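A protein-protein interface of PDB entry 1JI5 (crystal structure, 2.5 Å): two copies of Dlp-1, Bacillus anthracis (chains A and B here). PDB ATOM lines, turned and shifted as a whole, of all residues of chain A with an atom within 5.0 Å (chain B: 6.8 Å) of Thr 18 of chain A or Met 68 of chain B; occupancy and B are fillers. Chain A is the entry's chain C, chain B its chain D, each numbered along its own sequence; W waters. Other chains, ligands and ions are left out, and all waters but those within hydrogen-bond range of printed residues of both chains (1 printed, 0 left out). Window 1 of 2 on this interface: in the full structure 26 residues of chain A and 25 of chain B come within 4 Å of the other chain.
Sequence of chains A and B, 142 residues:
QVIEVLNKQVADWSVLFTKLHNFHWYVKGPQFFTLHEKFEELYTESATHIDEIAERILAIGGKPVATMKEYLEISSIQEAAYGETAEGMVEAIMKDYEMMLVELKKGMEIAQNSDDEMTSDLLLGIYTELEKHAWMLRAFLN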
ATOM      1  N   SER A  14       4.887  21.263 -19.713  1.00  0.00           N
ATOM      2  CA  SER A  14       3.535  20.797 -19.407  1.00  0.00           C
ATOM      3  C   SER A  14       2.902  21.670 -18.346  1.00  0.00           C
ATOM      4  O   SER A  14       1.715  21.987 -18.399  1.00  0.00           O
ATOM      5  CB  SER A  14       3.560  19.347 -18.935  1.00  0.00           C
ATOM      6  OG  SER A  14       4.008  18.493 -19.975  1.00  0.00           O
ATOM      7  N   VAL A  15       3.710  22.063 -17.375  1.00  0.00           N
ATOM      8  CA  VAL A  15       3.220  22.921 -16.312  1.00  0.00           C
ATOM      9  C   VAL A  15       2.924  24.301 -16.905  1.00  0.00           C
ATOM     10  O   VAL A  15       1.862  24.884 -16.658  1.00  0.00           O
ATOM     11  CB  VAL A  15       4.262  23.068 -15.172  1.00  0.00           C
ATOM     12  CG1 VAL A  15       3.657  23.877 -14.033  1.00  0.00           C
ATOM     13  CG2 VAL A  15       4.718  21.693 -14.682  1.00  0.00           C
ATOM     14  N   LEU A  16       3.869  24.823 -17.687  1.00  0.00           N
ATOM     15  CA  LEU A  16       3.678  26.119 -18.313  1.00  0.00           C
ATOM     16  C   LEU A  16       2.351  26.118 -19.069  1.00  0.00           C
ATOM     17  O   LEU A  16       1.584  27.074 -18.962  1.00  0.00           O
ATOM     18  CB  LEU A  16       4.823  26.441 -19.281  1.00  0.00           C
ATOM     19  CG  LEU A  16       6.002  27.326 -18.844  1.00  0.00           C
ATOM     20  CD1 LEU A  16       5.623  28.173 -17.640  1.00  0.00           C
ATOM     21  CD2 LEU A  16       7.195  26.451 -18.524  1.00  0.00           C
ATOM     22  N   PHE A  17       2.086  25.043 -19.818  1.00  0.00           N
ATOM     23  CA  PHE A  17       0.844  24.912 -20.599  1.00  0.00           C
ATOM     24  C   PHE A  17      -0.401  25.256 -19.768  1.00  0.00           C
ATOM     25  O   PHE A  17      -1.236  26.072 -20.169  1.00  0.00           O
ATOM     26  CB  PHE A  17       0.731  23.481 -21.158  1.00  0.00           C
ATOM     27  CG  PHE A  17      -0.525  23.216 -21.975  1.00  0.00           C
ATOM     28  CD1 PHE A  17      -1.628  22.572 -21.400  1.00  0.00           C
ATOM     29  CD2 PHE A  17      -0.580  23.546 -23.333  1.00  0.00           C
ATOM     30  CE1 PHE A  17      -2.764  22.252 -22.162  1.00  0.00           C
ATOM     31  CE2 PHE A  17      -1.708  23.231 -24.097  1.00  0.00           C
ATOM     32  CZ  PHE A  17      -2.802  22.578 -23.508  1.00  0.00           C
ATOM     33  N   THR A  18      -0.515  24.633 -18.602  1.00  0.00           N
ATOM     34  CA  THR A  18      -1.647  24.870 -17.718  1.00  0.00           C
ATOM     35  C   THR A  18      -1.567  26.272 -17.105  1.00  0.00           C
ATOM     36  O   THR A  18      -2.554  27.015 -17.075  1.00  0.00           O
ATOM     37  CB  THR A  18      -1.669  23.811 -16.584  1.00  0.00           C
ATOM     38  OG1 THR A  18      -1.574  22.504 -17.165  1.00  0.00           O
ATOM     39  CG2 THR A  18      -2.950  23.916 -15.744  1.00  0.00           C
ATOM     40  N   LYS A  19      -0.381  26.630 -16.619  1.00  0.00           N
ATOM     41  CA  LYS A  19      -0.175  27.927 -15.991  1.00  0.00           C
ATOM     42  C   LYS A  19      -0.536  29.074 -16.944  1.00  0.00           C
ATOM     43  O   LYS A  19      -1.092  30.099 -16.523  1.00  0.00           O
ATOM     44  CB  LYS A  19       1.282  28.041 -15.512  1.00  0.00           C
ATOM     45  CG  LYS A  19       1.540  29.184 -14.524  1.00  0.00           C
ATOM     46  CD  LYS A  19       2.940  29.112 -13.936  1.00  0.00           C
ATOM     47  CE  LYS A  19       3.241  30.319 -13.067  1.00  0.00           C
ATOM     48  NZ  LYS A  19       4.603  30.224 -12.451  1.00  0.00           N
ATOM     49  N   LEU A  20      -0.229  28.894 -18.228  1.00  0.00           N
ATOM     50  CA  LEU A  20      -0.526  29.904 -19.250  1.00  0.00           C
ATOM     51  C   LEU A  20      -2.018  29.975 -19.522  1.00  0.00           C
ATOM     52  O   LEU A  20      -2.536  31.041 -19.857  1.00  0.00           O
ATOM     53  CB  LEU A  20       0.224  29.593 -20.543  1.00  0.00           C
ATOM     54  CG  LEU A  20       1.721  29.892 -20.483  1.00  0.00           C
ATOM     55  CD1 LEU A  20       2.460  29.220 -21.633  1.00  0.00           C
ATOM     56  CD2 LEU A  20       1.904  31.404 -20.479  1.00  0.00           C
ATOM     57  N   HIS A  21      -2.702  28.840 -19.389  1.00  0.00           N
ATOM     58  CA  HIS A  21      -4.153  28.806 -19.567  1.00  0.00           C
ATOM     59  C   HIS A  21      -4.788  29.592 -18.428  1.00  0.00           C
ATOM     60  O   HIS A  21      -5.727  30.371 -18.632  1.00  0.00           O
ATOM     61  CB  HIS A  21      -4.684  27.392 -19.488  1.00  0.00           C
ATOM     62  CG  HIS A  21      -4.671  26.663 -20.785  1.00  0.00           C
ATOM     63  ND1 HIS A  21      -3.508  26.265 -21.404  1.00  0.00           N
ATOM     64  CD2 HIS A  21      -5.687  26.248 -21.578  1.00  0.00           C
ATOM     65  CE1 HIS A  21      -3.808  25.636 -22.526  1.00  0.00           C
ATOM     66  NE2 HIS A  21      -5.124  25.610 -22.655  1.00  0.00           N
ATOM     67  N   ASN A  22      -4.277  29.347 -17.219  1.00  0.00           N
ATOM     68  CA  ASN A  22      -4.744  30.020 -16.014  1.00  0.00           C
ATOM     69  C   ASN A  22      -4.692  31.522 -16.252  1.00  0.00           C
ATOM     70  O   ASN A  22      -5.705  32.216 -16.124  1.00  0.00           O
ATOM     71  CB  ASN A  22      -3.845  29.653 -14.827  1.00  0.00           C
ATOM     72  CG  ASN A  22      -4.312  30.285 -13.501  1.00  0.00           C
ATOM     73  OD1 ASN A  22      -4.291  31.510 -13.336  1.00  0.00           O
ATOM     74  ND2 ASN A  22      -4.728  29.437 -12.549  1.00  0.00           N
ATOM     75  N   MET A  68       0.626  13.626 -15.592  1.00  0.00           N
ATOM     76  CA  MET A  68       0.702  14.881 -14.887  1.00  0.00           C
ATOM     77  C   MET A  68       1.349  14.612 -13.544  1.00  0.00           C
ATOM     78  O   MET A  68       2.070  15.455 -13.012  1.00  0.00           O
ATOM     79  CB  MET A  68      -0.692  15.452 -14.699  1.00  0.00           C
ATOM     80  CG  MET A  68      -1.365  15.767 -16.007  1.00  0.00           C
ATOM     81  SD  MET A  68      -3.040  16.307 -15.759  1.00  0.00           S
ATOM     82  CE  MET A  68      -2.801  17.909 -15.172  1.00  0.00           C
ATOM     83  N   TYR A  71       5.021  14.800 -13.945  1.00  0.00           N
ATOM     84  CA  TYR A  71       5.319  16.199 -14.239  1.00  0.00           C
ATOM     85  C   TYR A  71       5.436  16.996 -12.949  1.00  0.00           C
ATOM     86  O   TYR A  71       6.419  17.709 -12.732  1.00  0.00           O
ATOM     87  CB  TYR A  71       4.225  16.813 -15.130  1.00  0.00           C
ATOM     88  CG  TYR A  71       4.170  16.236 -16.526  1.00  0.00           C
ATOM     89  CD1 TYR A  71       2.954  16.103 -17.199  1.00  0.00           C
ATOM     90  CD2 TYR A  71       5.334  15.799 -17.174  1.00  0.00           C
ATOM     91  CE1 TYR A  71       2.895  15.542 -18.479  1.00  0.00           C
ATOM     92  CE2 TYR A  71       5.287  15.242 -18.451  1.00  0.00           C
ATOM     93  CZ  TYR A  71       4.067  15.114 -19.095  1.00  0.00           C
ATOM     94  OH  TYR A  71       4.014  14.550 -20.344  1.00  0.00           O
ATOM     95  N   LEU A  72       4.428  16.858 -12.092  1.00  0.00           N
ATOM     96  CA  LEU A  72       4.386  17.578 -10.826  1.00  0.00           C
ATOM     97  C   LEU A  72       5.574  17.256  -9.916  1.00  0.00           C
ATOM     98  O   LEU A  72       6.153  18.151  -9.297  1.00  0.00           O
ATOM     99  CB  LEU A  72       3.062  17.288 -10.106  1.00  0.00           C
ATOM    100  CG  LEU A  72       1.917  18.321 -10.095  1.00  0.00           C
ATOM    101  CD1 LEU A  72       2.150  19.421 -11.112  1.00  0.00           C
ATOM    102  CD2 LEU A  72       0.594  17.608 -10.377  1.00  0.00           C
ATOM    103  N   GLU A  79       3.404  26.215  -9.943  1.00  0.00           N
ATOM    104  CA  GLU A  79       2.049  26.250 -10.477  1.00  0.00           C
ATOM    105  C   GLU A  79       1.413  27.545 -10.004  1.00  0.00           C
ATOM    106  O   GLU A  79       1.629  27.985  -8.883  1.00  0.00           O
ATOM    107  CB  GLU A  79       1.250  25.054  -9.974  1.00  0.00           C
ATOM    108  CG  GLU A  79      -0.003  24.779 -10.754  1.00  0.00           C
ATOM    109  CD  GLU A  79      -0.157  23.306 -11.085  1.00  0.00           C
ATOM    110  OE1 GLU A  79      -0.344  22.496 -10.155  1.00  0.00           O
ATOM    111  OE2 GLU A  79      -0.084  22.951 -12.278  1.00  0.00           O
ATOM    112  N   SER B  14      -8.220  17.804 -19.271  1.00  0.00           N
ATOM    113  CA  SER B  14      -6.808  18.093 -19.076  1.00  0.00           C
ATOM    114  C   SER B  14      -6.038  16.798 -18.950  1.00  0.00           C
ATOM    115  O   SER B  14      -4.920  16.674 -19.453  1.00  0.00           O
ATOM    116  CB  SER B  14      -6.604  18.932 -17.827  1.00  0.00           C
ATOM    117  OG  SER B  14      -7.207  20.201 -17.969  1.00  0.00           O
ATOM    118  N   THR B  18      -3.002  14.894 -21.693  1.00  0.00           N
ATOM    119  CA  THR B  18      -1.725  14.256 -21.425  1.00  0.00           C
ATOM    120  C   THR B  18      -1.759  12.778 -21.811  1.00  0.00           C
ATOM    121  O   THR B  18      -0.845  12.260 -22.473  1.00  0.00           O
ATOM    122  CB  THR B  18      -1.373  14.382 -19.930  1.00  0.00           C
ATOM    123  OG1 THR B  18      -1.537  15.747 -19.523  1.00  0.00           O
ATOM    124  CG2 THR B  18       0.069  13.936 -19.667  1.00  0.00           C
ATOM    125  N   VAL B  65     -10.919  25.715 -12.535  1.00  0.00           N
ATOM    126  CA  VAL B  65      -9.781  25.093 -11.876  1.00  0.00           C
ATOM    127  C   VAL B  65      -8.620  25.263 -12.845  1.00  0.00           C
ATOM    128  O   VAL B  65      -8.788  25.070 -14.048  1.00  0.00           O
ATOM    129  CB  VAL B  65     -10.029  23.591 -11.633  1.00  0.00           C
ATOM    130  CG1 VAL B  65     -11.034  23.408 -10.500  1.00  0.00           C
ATOM    131  CG2 VAL B  65     -10.559  22.941 -12.910  1.00  0.00           C
ATOM    132  N   ALA B  66      -7.447  25.625 -12.339  1.00  0.00           N
ATOM    133  CA  ALA B  66      -6.325  25.831 -13.234  1.00  0.00           C
ATOM    134  C   ALA B  66      -4.945  25.431 -12.717  1.00  0.00           C
ATOM    135  O   ALA B  66      -3.992  26.210 -12.790  1.00  0.00           O
ATOM    136  CB  ALA B  66      -6.314  27.273 -13.699  1.00  0.00           C
ATOM    137  N   THR B  67      -4.843  24.217 -12.189  1.00  0.00           N
ATOM    138  CA  THR B  67      -3.565  23.678 -11.729  1.00  0.00           C
ATOM    139  C   THR B  67      -3.659  22.182 -11.964  1.00  0.00           C
ATOM    140  O   THR B  67      -4.723  21.588 -11.810  1.00  0.00           O
ATOM    141  CB  THR B  67      -3.274  23.944 -10.217  1.00  0.00           C
ATOM    142  OG1 THR B  67      -4.273  23.315  -9.399  1.00  0.00           O
ATOM    143  CG2 THR B  67      -3.224  25.438  -9.939  1.00  0.00           C
ATOM    144  N   MET B  68      -2.561  21.574 -12.374  1.00  0.00           N
ATOM    145  CA  MET B  68      -2.578  20.149 -12.611  1.00  0.00           C
ATOM    146  C   MET B  68      -2.888  19.478 -11.285  1.00  0.00           C
ATOM    147  O   MET B  68      -3.541  18.431 -11.249  1.00  0.00           O
ATOM    148  CB  MET B  68      -1.226  19.708 -13.149  1.00  0.00           C
ATOM    149  CG  MET B  68      -0.910  20.347 -14.485  1.00  0.00           C
ATOM    150  SD  MET B  68       0.722  19.969 -15.075  1.00  0.00           S
ATOM    151  CE  MET B  68       0.546  18.284 -15.491  1.00  0.00           C
ATOM    152  N   LYS B  69      -2.435  20.107 -10.199  1.00  0.00           N
ATOM    153  CA  LYS B  69      -2.660  19.595  -8.855  1.00  0.00           C
ATOM    154  C   LYS B  69      -4.143  19.342  -8.623  1.00  0.00           C
ATOM    155  O   LYS B  69      -4.542  18.237  -8.254  1.00  0.00           O
ATOM    156  CB  LYS B  69      -2.149  20.586  -7.815  1.00  0.00           C
ATOM    157  CG  LYS B  69      -2.529  20.206  -6.384  1.00  0.00           C
ATOM    158  CD  LYS B  69      -2.304  21.365  -5.411  1.00  0.00           C
ATOM    159  CE  LYS B  69      -2.865  21.056  -4.022  1.00  0.00           C
ATOM    160  NZ  LYS B  69      -2.246  19.830  -3.436  1.00  0.00           N
ATOM    161  N   GLU B  70      -4.959  20.366  -8.838  1.00  0.00           N
ATOM    162  CA  GLU B  70      -6.395  20.223  -8.648  1.00  0.00           C
ATOM    163  C   GLU B  70      -6.958  19.197  -9.619  1.00  0.00           C
ATOM    164  O   GLU B  70      -7.712  18.318  -9.221  1.00  0.00           O
ATOM    165  CB  GLU B  70      -7.081  21.572  -8.828  1.00  0.00           C
ATOM    166  CG  GLU B  70      -6.550  22.605  -7.869  1.00  0.00           C
ATOM    167  CD  GLU B  70      -7.201  23.953  -8.031  1.00  0.00           C
ATOM    168  OE1 GLU B  70      -8.386  24.104  -7.658  1.00  0.00           O
ATOM    169  OE2 GLU B  70      -6.518  24.868  -8.534  1.00  0.00           O
ATOM    170  N   TYR B  71      -6.564  19.296 -10.886  1.00  0.00           N
ATOM    171  CA  TYR B  71      -7.025  18.365 -11.914  1.00  0.00           C
ATOM    172  C   TYR B  71      -6.919  16.931 -11.421  1.00  0.00           C
ATOM    173  O   TYR B  71      -7.879  16.159 -11.499  1.00  0.00           O
ATOM    174  CB  TYR B  71      -6.189  18.527 -13.183  1.00  0.00           C
ATOM    175  CG  TYR B  71      -6.420  19.832 -13.913  1.00  0.00           C
ATOM    176  CD1 TYR B  71      -5.398  20.428 -14.644  1.00  0.00           C
ATOM    177  CD2 TYR B  71      -7.653  20.478 -13.862  1.00  0.00           C
ATOM    178  CE1 TYR B  71      -5.591  21.637 -15.301  1.00  0.00           C
ATOM    179  CE2 TYR B  71      -7.857  21.686 -14.516  1.00  0.00           C
ATOM    180  CZ  TYR B  71      -6.817  22.260 -15.233  1.00  0.00           C
ATOM    181  OH  TYR B  71      -6.993  23.462 -15.876  1.00  0.00           O
ATOM    182  N   LEU B  72      -5.741  16.594 -10.903  1.00  0.00           N
ATOM    183  CA  LEU B  72      -5.464  15.260 -10.397  1.00  0.00           C
ATOM    184  C   LEU B  72      -6.390  14.855  -9.244  1.00  0.00           C
ATOM    185  O   LEU B  72      -6.878  13.724  -9.199  1.00  0.00           O
ATOM    186  CB  LEU B  72      -3.993  15.177  -9.976  1.00  0.00           C
ATOM    187  CG  LEU B  72      -2.984  14.416 -10.859  1.00  0.00           C
ATOM    188  CD1 LEU B  72      -3.521  14.154 -12.250  1.00  0.00           C
ATOM    189  CD2 LEU B  72      -1.696  15.211 -10.927  1.00  0.00           C
ATOM    190  N   GLU B  73      -6.656  15.770  -8.321  1.00  0.00           N
ATOM    191  CA  GLU B  73      -7.530  15.423  -7.211  1.00  0.00           C
ATOM    192  C   GLU B  73      -9.025  15.460  -7.539  1.00  0.00           C
ATOM    193  O   GLU B  73      -9.849  15.102  -6.696  1.00  0.00           O
ATOM    194  CB  GLU B  73      -7.215  16.290  -5.976  1.00  0.00           C
ATOM    195  CG  GLU B  73      -6.990  17.758  -6.251  1.00  0.00           C
ATOM    196  CD  GLU B  73      -6.293  18.467  -5.094  1.00  0.00           C
ATOM    197  OE1 GLU B  73      -5.257  17.950  -4.615  1.00  0.00           O
ATOM    198  OE2 GLU B  73      -6.772  19.547  -4.674  1.00  0.00           O
ATOM    199  N   GLU B  79      -4.962   8.083 -15.413  1.00  0.00           N
ATOM    200  CA  GLU B  79      -3.817   8.319 -16.294  1.00  0.00           C
ATOM    201  C   GLU B  79      -3.259   7.020 -16.856  1.00  0.00           C
ATOM    202  O   GLU B  79      -3.621   5.921 -16.410  1.00  0.00           O
ATOM    203  CB  GLU B  79      -2.681   9.071 -15.576  1.00  0.00           C
ATOM    204  CG  GLU B  79      -3.002  10.489 -15.130  1.00  0.00           C
ATOM    205  CD  GLU B  79      -1.760  11.288 -14.762  1.00  0.00           C
ATOM    206  OE1 GLU B  79      -1.343  12.162 -15.545  1.00  0.00           O
ATOM    207  OE2 GLU B  79      -1.190  11.042 -13.691  1.00  0.00           O
HETATM  208  O   HOH W   1      -4.154  21.286 -18.832  1.00  0.00           O
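The backbone NH (N) of Met 68 of chain A lies within hydrogen-bond range of the side-chain carboxylate (OE1) of Glu 79 of chain B, 2.5 Å away. The side-chain amide nitrogen (ND2) of Asn 22 of chain A sits close to the backbone carbonyl oxygen (O) of Ala 66 of chain B (3.3 Å). The side-chain carboxylate of Glu 79 of chain A lies within hydrogen-bond range of the backbone NH of Lys 69 of chain B, 3.2 Å away. OE2 of Glu 79 of chain A is in hydrogen-bond range of N of Met 68 of chain B.
The side-chain hydroxyl of Thr 67 of chain B lies close to the side-chain carboxylate of Glu 70 of chain B (2.9 Å). The side-chain carboxylate (OE1) of Glu 73 of chain B lies within salt-bridge range of the side-chain amino group (NZ) of Lys 69 of chain B (3.7 Å). The side-chain hydroxyl (OH) of Tyr 71 of chain B is in hydrogen-bond range of the backbone carbonyl oxygen (O) of Val 65 of chain B (3.0 Å).
Thr 18 of chain A touches Ala 66 of chain B (CG2 to O, 3.9 Å). Thr 18 of chain A touches Met 68 of chain B (OG1 to CG, 3.5 Å). Tyr 71 of chain B touches Thr 18 of chain A. CG of Met 68 of chain A touches OG1 of Thr 18 of chain B, at 3.5 Å. Tyr 71 of chain B touches Met 68 of chain A (CD1 to CE, 3.7 Å). Met 68 of chain A touches Leu 72 of chain B (CB to CD2, 3.9 Å). CE1 of Tyr 71 of chain A touches CG2 of Thr 18 of chain B, at 3.5 Å. Tyr 71 of chain A touches Met 68 of chain B (CD1 to CE, 3.7 Å). Leu 72 of chain A touches Met 68 of chain B. Leu 72 of chain B touches Leu 72 of chain A (CD2 to CD2, 3.4 Å).
Printed residues of chain B within 4 Å of Thr 18 of chain A: Ala 66 (3.9 Å), Met 68 (3.5 Å) and Tyr 71 (3.5 Å). Of the printed residues of chain A, Met 68 of chain B touches Thr 18 (3.5 Å), Met 68 (3.1 Å), Tyr 71 (3.7 Å), Leu 72 (3.9 Å) and Glu 79 (2.8 Å). Of the printed residues of chain B, Glu 79 of chain A touches Thr 67 (3.3 Å), Met 68 (2.8 Å) and Lys 69 (3.2 Å). Printed residues of chain A within 4 Å of Lys 69 of chain B: Leu 72 (3.9 Å) and Glu 79 (3.2 Å). Val 15 of chain A touches none of the printed residues of chain B. The nearest residue of chain B that does not touch Thr 18 of chain A is Thr 67 of chain B (4.04 Å). The nearest printed residue of chain B that does not touch Tyr 71 of chain A is Glu 79 of chain B (6.1 Å).
Hydrophobic or aromatic side chains of chain A within 4 Å of the printed part of chain B: Met 68, Tyr 71 and Leu 72. Of the 12 printed residues of chain B, 8 touch a printed residue of chain A. Among the printed residues, no Asp or Glu carboxylate lies within 4 Å of a Lys or Arg side-chain nitrogen of the other chain.
Thr 18 of chain A touches Tyr 71 of chain B, and with the chains exchanged Tyr 71 of chain A touches Thr 18 of chain B. Met 68 of chain A touches its own counterpart, Met 68 of chain B. Met 68 of chain A touches Tyr 71 of chain B, and with the chains exchanged Tyr 71 of chain A touches Met 68 of chain B. Leu 72 of chain B touches its own counterpart, Leu 72 of chain A. Of the 17 pairs that touch across the chains among the printed residues, 12 have their exchanged pair printed and touching as well.
Water W1 lies within hydrogen-bond range of the side-chain hydroxyl of Thr 18 of chain A (3.3 Å) and the side-chain hydroxyl of Ser 14 of chain B (3.4 Å).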
